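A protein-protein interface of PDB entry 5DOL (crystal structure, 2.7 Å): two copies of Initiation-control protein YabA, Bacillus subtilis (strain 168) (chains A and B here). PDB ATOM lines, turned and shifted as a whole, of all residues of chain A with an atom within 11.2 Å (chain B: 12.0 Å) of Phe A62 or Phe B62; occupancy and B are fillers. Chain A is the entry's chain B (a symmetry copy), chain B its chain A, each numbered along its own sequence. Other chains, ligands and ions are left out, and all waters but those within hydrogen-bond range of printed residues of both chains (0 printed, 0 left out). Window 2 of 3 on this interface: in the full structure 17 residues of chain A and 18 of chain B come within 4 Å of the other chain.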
ATOM      1  N   ASP A  54     -21.119  -7.139 -24.835  1.00  0.00           N
ATOM      2  CA  ASP A  54     -20.760  -7.405 -26.227  1.00  0.00           C
ATOM      3  C   ASP A  54     -19.357  -6.893 -26.572  1.00  0.00           C
ATOM      4  O   ASP A  54     -18.564  -7.607 -27.192  1.00  0.00           O
ATOM      5  CB  ASP A  54     -21.791  -6.784 -27.177  1.00  0.00           C
ATOM      6  N   THR A  55     -19.054  -5.665 -26.158  1.00  0.00           N
ATOM      7  CA  THR A  55     -17.767  -5.052 -26.476  1.00  0.00           C
ATOM      8  C   THR A  55     -16.623  -5.726 -25.707  1.00  0.00           C
ATOM      9  O   THR A  55     -15.491  -5.803 -26.200  1.00  0.00           O
ATOM     10  CB  THR A  55     -17.783  -3.527 -26.189  1.00  0.00           C
ATOM     11  OG1 THR A  55     -16.617  -2.911 -26.751  1.00  0.00           O
ATOM     12  CG2 THR A  55     -17.826  -3.247 -24.701  1.00  0.00           C
ATOM     13  N   THR A  56     -16.916  -6.231 -24.512  1.00  0.00           N
ATOM     14  CA  THR A  56     -15.913  -6.976 -23.764  1.00  0.00           C
ATOM     15  C   THR A  56     -15.689  -8.333 -24.417  1.00  0.00           C
ATOM     16  O   THR A  56     -14.584  -8.874 -24.376  1.00  0.00           O
ATOM     17  CB  THR A  56     -16.306  -7.163 -22.288  1.00  0.00           C
ATOM     18  OG1 THR A  56     -17.688  -7.529 -22.197  1.00  0.00           O
ATOM     19  CG2 THR A  56     -16.071  -5.875 -21.513  1.00  0.00           C
ATOM     20  N   GLN A  57     -16.738  -8.879 -25.027  1.00  0.00           N
ATOM     21  CA  GLN A  57     -16.596 -10.108 -25.806  1.00  0.00           C
ATOM     22  C   GLN A  57     -15.781  -9.854 -27.080  1.00  0.00           C
ATOM     23  O   GLN A  57     -15.079 -10.744 -27.558  1.00  0.00           O
ATOM     24  CB  GLN A  57     -17.966 -10.697 -26.161  1.00  0.00           C
ATOM     25  CG  GLN A  57     -18.703 -11.325 -24.985  1.00  0.00           C
ATOM     26  N   GLN A  58     -15.874  -8.642 -27.622  1.00  0.00           N
ATOM     27  CA  GLN A  58     -15.092  -8.277 -28.804  1.00  0.00           C
ATOM     28  C   GLN A  58     -13.612  -8.091 -28.476  1.00  0.00           C
ATOM     29  O   GLN A  58     -12.749  -8.629 -29.168  1.00  0.00           O
ATOM     30  CB  GLN A  58     -15.632  -6.997 -29.451  1.00  0.00           C
ATOM     31  CG  GLN A  58     -17.035  -7.111 -30.039  1.00  0.00           C
ATOM     32  CD  GLN A  58     -17.445  -5.870 -30.814  1.00  0.00           C
ATOM     33  OE1 GLN A  58     -16.595  -5.094 -31.254  1.00  0.00           O
ATOM     34  NE2 GLN A  58     -18.751  -5.675 -30.981  1.00  0.00           N
ATOM     35  N   ILE A  59     -13.320  -7.324 -27.428  1.00  0.00           N
ATOM     36  CA  ILE A  59     -11.929  -7.056 -27.060  1.00  0.00           C
ATOM     37  C   ILE A  59     -11.189  -8.327 -26.645  1.00  0.00           C
ATOM     38  O   ILE A  59     -10.066  -8.572 -27.088  1.00  0.00           O
ATOM     39  CB  ILE A  59     -11.827  -6.020 -25.916  1.00  0.00           C
ATOM     40  CG1 ILE A  59     -12.185  -4.625 -26.426  1.00  0.00           C
ATOM     41  CG2 ILE A  59     -10.421  -5.999 -25.331  1.00  0.00           C
ATOM     42  CD1 ILE A  59     -11.762  -3.507 -25.492  1.00  0.00           C
ATOM     43  N   GLU A  60     -11.832  -9.145 -25.816  1.00  0.00           N
ATOM     44  CA  GLU A  60     -11.210 -10.362 -25.293  1.00  0.00           C
ATOM     45  C   GLU A  60     -11.059 -11.454 -26.361  1.00  0.00           C
ATOM     46  O   GLU A  60     -10.685 -12.587 -26.054  1.00  0.00           O
ATOM     47  CB  GLU A  60     -12.011 -10.889 -24.099  1.00  0.00           C
ATOM     48  N   LYS A  61     -11.353 -11.106 -27.611  1.00  0.00           N
ATOM     49  CA  LYS A  61     -11.106 -11.994 -28.742  1.00  0.00           C
ATOM     50  C   LYS A  61     -10.060 -11.337 -29.642  1.00  0.00           C
ATOM     51  O   LYS A  61      -9.716 -11.858 -30.705  1.00  0.00           O
ATOM     52  CB  LYS A  61     -12.403 -12.282 -29.509  1.00  0.00           C
ATOM     53  N   PHE A  62      -9.556 -10.189 -29.187  1.00  0.00           N
ATOM     54  CA  PHE A  62      -8.510  -9.437 -29.881  1.00  0.00           C
ATOM     55  C   PHE A  62      -8.968  -8.992 -31.266  1.00  0.00           C
ATOM     56  O   PHE A  62      -9.439  -7.869 -31.448  1.00  0.00           O
ATOM     57  CB  PHE A  62      -7.223 -10.265 -29.995  1.00  0.00           C
ATOM     58  CG  PHE A  62      -6.858 -10.999 -28.739  1.00  0.00           C
ATOM     59  CD1 PHE A  62      -6.345 -10.316 -27.654  1.00  0.00           C
ATOM     60  CD2 PHE A  62      -7.017 -12.372 -28.648  1.00  0.00           C
ATOM     61  CE1 PHE A  62      -6.005 -10.981 -26.496  1.00  0.00           C
ATOM     62  CE2 PHE A  62      -6.680 -13.042 -27.497  1.00  0.00           C
ATOM     63  CZ  PHE A  62      -6.173 -12.350 -26.420  1.00  0.00           C
ATOM     64  N   ARG B  51     -16.940   3.431 -18.852  1.00  0.00           N
ATOM     65  CA  ARG B  51     -16.419   2.122 -19.238  1.00  0.00           C
ATOM     66  C   ARG B  51     -16.595   1.894 -20.734  1.00  0.00           C
ATOM     67  O   ARG B  51     -15.666   1.465 -21.414  1.00  0.00           O
ATOM     68  CB  ARG B  51     -17.117   1.011 -18.449  1.00  0.00           C
ATOM     69  CG  ARG B  51     -16.521  -0.385 -18.644  1.00  0.00           C
ATOM     70  CD  ARG B  51     -15.391  -0.673 -17.658  1.00  0.00           C
ATOM     71  NE  ARG B  51     -14.074  -0.425 -18.229  1.00  0.00           N
ATOM     72  CZ  ARG B  51     -13.335  -1.353 -18.832  1.00  0.00           C
ATOM     73  NH1 ARG B  51     -13.787  -2.594 -18.940  1.00  0.00           N
ATOM     74  NH2 ARG B  51     -12.140  -1.042 -19.326  1.00  0.00           N
ATOM     75  N   ASP B  53     -16.977   4.181 -23.032  1.00  0.00           N
ATOM     76  CA  ASP B  53     -16.121   5.117 -23.751  1.00  0.00           C
ATOM     77  C   ASP B  53     -14.695   4.579 -23.836  1.00  0.00           C
ATOM     78  O   ASP B  53     -14.086   4.567 -24.909  1.00  0.00           O
ATOM     79  CB  ASP B  53     -16.134   6.494 -23.077  1.00  0.00           C
ATOM     80  CG  ASP B  53     -16.821   7.553 -23.922  1.00  0.00           C
ATOM     81  OD1 ASP B  53     -17.693   7.190 -24.740  1.00  0.00           O
ATOM     82  OD2 ASP B  53     -16.489   8.747 -23.769  1.00  0.00           O
ATOM     83  N   ASP B  54     -14.176   4.123 -22.700  1.00  0.00           N
ATOM     84  CA  ASP B  54     -12.820   3.590 -22.634  1.00  0.00           C
ATOM     85  C   ASP B  54     -12.643   2.359 -23.518  1.00  0.00           C
ATOM     86  O   ASP B  54     -11.650   2.244 -24.245  1.00  0.00           O
ATOM     87  CB  ASP B  54     -12.454   3.248 -21.191  1.00  0.00           C
ATOM     88  CG  ASP B  54     -12.442   4.464 -20.294  1.00  0.00           C
ATOM     89  OD1 ASP B  54     -12.923   5.529 -20.737  1.00  0.00           O
ATOM     90  OD2 ASP B  54     -11.962   4.357 -19.146  1.00  0.00           O
ATOM     91  N   THR B  55     -13.608   1.446 -23.457  1.00  0.00           N
ATOM     92  CA  THR B  55     -13.535   0.213 -24.227  1.00  0.00           C
ATOM     93  C   THR B  55     -13.720   0.512 -25.727  1.00  0.00           C
ATOM     94  O   THR B  55     -13.142  -0.169 -26.587  1.00  0.00           O
ATOM     95  CB  THR B  55     -14.581  -0.823 -23.727  1.00  0.00           C
ATOM     96  OG1 THR B  55     -14.365  -2.084 -24.367  1.00  0.00           O
ATOM     97  CG2 THR B  55     -15.969  -0.374 -24.024  1.00  0.00           C
ATOM     98  N   THR B  56     -14.499   1.552 -26.031  1.00  0.00           N
ATOM     99  CA  THR B  56     -14.698   1.990 -27.411  1.00  0.00           C
ATOM    100  C   THR B  56     -13.408   2.567 -27.981  1.00  0.00           C
ATOM    101  O   THR B  56     -13.052   2.290 -29.125  1.00  0.00           O
ATOM    102  CB  THR B  56     -15.817   3.044 -27.531  1.00  0.00           C
ATOM    103  OG1 THR B  56     -17.064   2.468 -27.123  1.00  0.00           O
ATOM    104  CG2 THR B  56     -15.946   3.531 -28.966  1.00  0.00           C
ATOM    105  N   GLN B  57     -12.711   3.371 -27.182  1.00  0.00           N
ATOM    106  CA  GLN B  57     -11.422   3.901 -27.604  1.00  0.00           C
ATOM    107  C   GLN B  57     -10.409   2.767 -27.777  1.00  0.00           C
ATOM    108  O   GLN B  57      -9.625   2.760 -28.735  1.00  0.00           O
ATOM    109  CB  GLN B  57     -10.912   4.942 -26.604  1.00  0.00           C
ATOM    110  N   GLN B  58     -10.445   1.804 -26.857  1.00  0.00           N
ATOM    111  CA  GLN B  58      -9.595   0.617 -26.945  1.00  0.00           C
ATOM    112  C   GLN B  58      -9.811  -0.135 -28.254  1.00  0.00           C
ATOM    113  O   GLN B  58      -8.850  -0.577 -28.886  1.00  0.00           O
ATOM    114  CB  GLN B  58      -9.850  -0.331 -25.771  1.00  0.00           C
ATOM    115  CG  GLN B  58      -8.792  -0.294 -24.680  1.00  0.00           C
ATOM    116  CD  GLN B  58      -8.908   0.930 -23.798  1.00  0.00           C
ATOM    117  OE1 GLN B  58      -8.442   2.012 -24.152  1.00  0.00           O
ATOM    118  NE2 GLN B  58      -9.539   0.767 -22.640  1.00  0.00           N
ATOM    119  N   ILE B  59     -11.072  -0.290 -28.655  1.00  0.00           N
ATOM    120  CA  ILE B  59     -11.372  -0.953 -29.922  1.00  0.00           C
ATOM    121  C   ILE B  59     -10.944  -0.080 -31.108  1.00  0.00           C
ATOM    122  O   ILE B  59     -10.480  -0.594 -32.126  1.00  0.00           O
ATOM    123  CB  ILE B  59     -12.872  -1.310 -30.043  1.00  0.00           C
ATOM    124  CG1 ILE B  59     -13.228  -2.433 -29.068  1.00  0.00           C
ATOM    125  CG2 ILE B  59     -13.223  -1.738 -31.463  1.00  0.00           C
ATOM    126  CD1 ILE B  59     -14.594  -3.055 -29.307  1.00  0.00           C
ATOM    127  N   GLU B  60     -11.078   1.238 -30.962  1.00  0.00           N
ATOM    128  CA  GLU B  60     -10.673   2.171 -32.012  1.00  0.00           C
ATOM    129  C   GLU B  60      -9.168   2.084 -32.246  1.00  0.00           C
ATOM    130  O   GLU B  60      -8.690   2.328 -33.357  1.00  0.00           O
ATOM    131  CB  GLU B  60     -11.071   3.608 -31.665  1.00  0.00           C
ATOM    132  N   LYS B  61      -8.423   1.741 -31.197  1.00  0.00           N
ATOM    133  CA  LYS B  61      -7.004   1.444 -31.363  1.00  0.00           C
ATOM    134  C   LYS B  61      -6.844   0.149 -32.158  1.00  0.00           C
ATOM    135  O   LYS B  61      -6.288   0.149 -33.258  1.00  0.00           O
ATOM    136  N   PHE B  62      -7.336  -0.952 -31.599  1.00  0.00           N
ATOM    137  CA  PHE B  62      -7.351  -2.228 -32.311  1.00  0.00           C
ATOM    138  C   PHE B  62      -8.585  -3.057 -31.971  1.00  0.00           C
ATOM    139  O   PHE B  62      -8.548  -4.288 -32.017  1.00  0.00           O
ATOM    140  CB  PHE B  62      -6.083  -3.034 -32.013  1.00  0.00           C
ATOM    141  CG  PHE B  62      -5.651  -2.997 -30.570  1.00  0.00           C
ATOM    142  CD1 PHE B  62      -4.440  -2.425 -30.217  1.00  0.00           C
ATOM    143  CD2 PHE B  62      -6.446  -3.540 -29.572  1.00  0.00           C
ATOM    144  CE1 PHE B  62      -4.030  -2.390 -28.896  1.00  0.00           C
ATOM    145  CE2 PHE B  62      -6.042  -3.505 -28.248  1.00  0.00           C
ATOM    146  CZ  PHE B  62      -4.832  -2.929 -27.911  1.00  0.00           C
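Thr B55 touches its own counterpart, Thr A55.
Gln A58 touches Ile B59, and with the chains exchanged Ile A59 touches Gln B58.
Ile B59 touches its own counterpart, Ile A59.
Phe A62 touches its own counterpart, Phe B62.
Gln A57 touches none of the printed residues of chain B.
Of the printed residues of chain B, Gln A58 touches Ile B59 (3.5 Å).
No residue of chain B comes within 4 Å of Lys A61.
Phe A62 touches just one residue of chain B: Phe B62 (3.7 Å).
Printed residues of chain A within 4 Å of Thr B55: Thr A55 (3.4 Å) and Ile A59 (3.2 Å).
Gln B57 touches none of the printed residues of chain A.
Of the printed residues of chain A, Gln B58 touches Ile A59 (3.7 Å).
Ile B59 touches just these residues of chain A: Thr A55 (3.3 Å), Gln A58 (3.5 Å) and Ile A59 (3.6 Å).
Phe B62 touches just one residue of chain A: Phe A62 (3.7 Å).
The nearest residue of chain A that does not touch Phe B62 is Ile A59 (5.8 Å).
The nearest printed residue of chain A that does not touch Gln B58 is Thr A55 (7.3 Å).
Of the 9 printed residues of chain A, 4 touch a printed residue of chain B.
Of the 11 printed residues of chain B, 4 touch a printed residue of chain A.
Among the printed residues, 7 pairs touch across the chains.
The side-chain amide nitrogen of Gln B58 lies within hydrogen-bond range of the backbone carbonyl oxygen of Asp B54, 3.0 Å away.
Among the printed residues, merely in contact across the chains: Ile A59 with Thr B55 (3.2 Å), Thr A55 with Ile B59 (3.3 Å), Gln A58 with Ile B59 (3.5 Å), Ile A59 with Ile B59 (3.6 Å), Ile A59 with Gln B58 (3.7 Å) and Phe A62 with Phe B62 (3.7 Å).
The side-chain hydroxyl (OG1) of Thr A55 sits at hydrogen-bond distance from the side-chain hydroxyl (OG1) of Thr B55 (3.4 Å).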
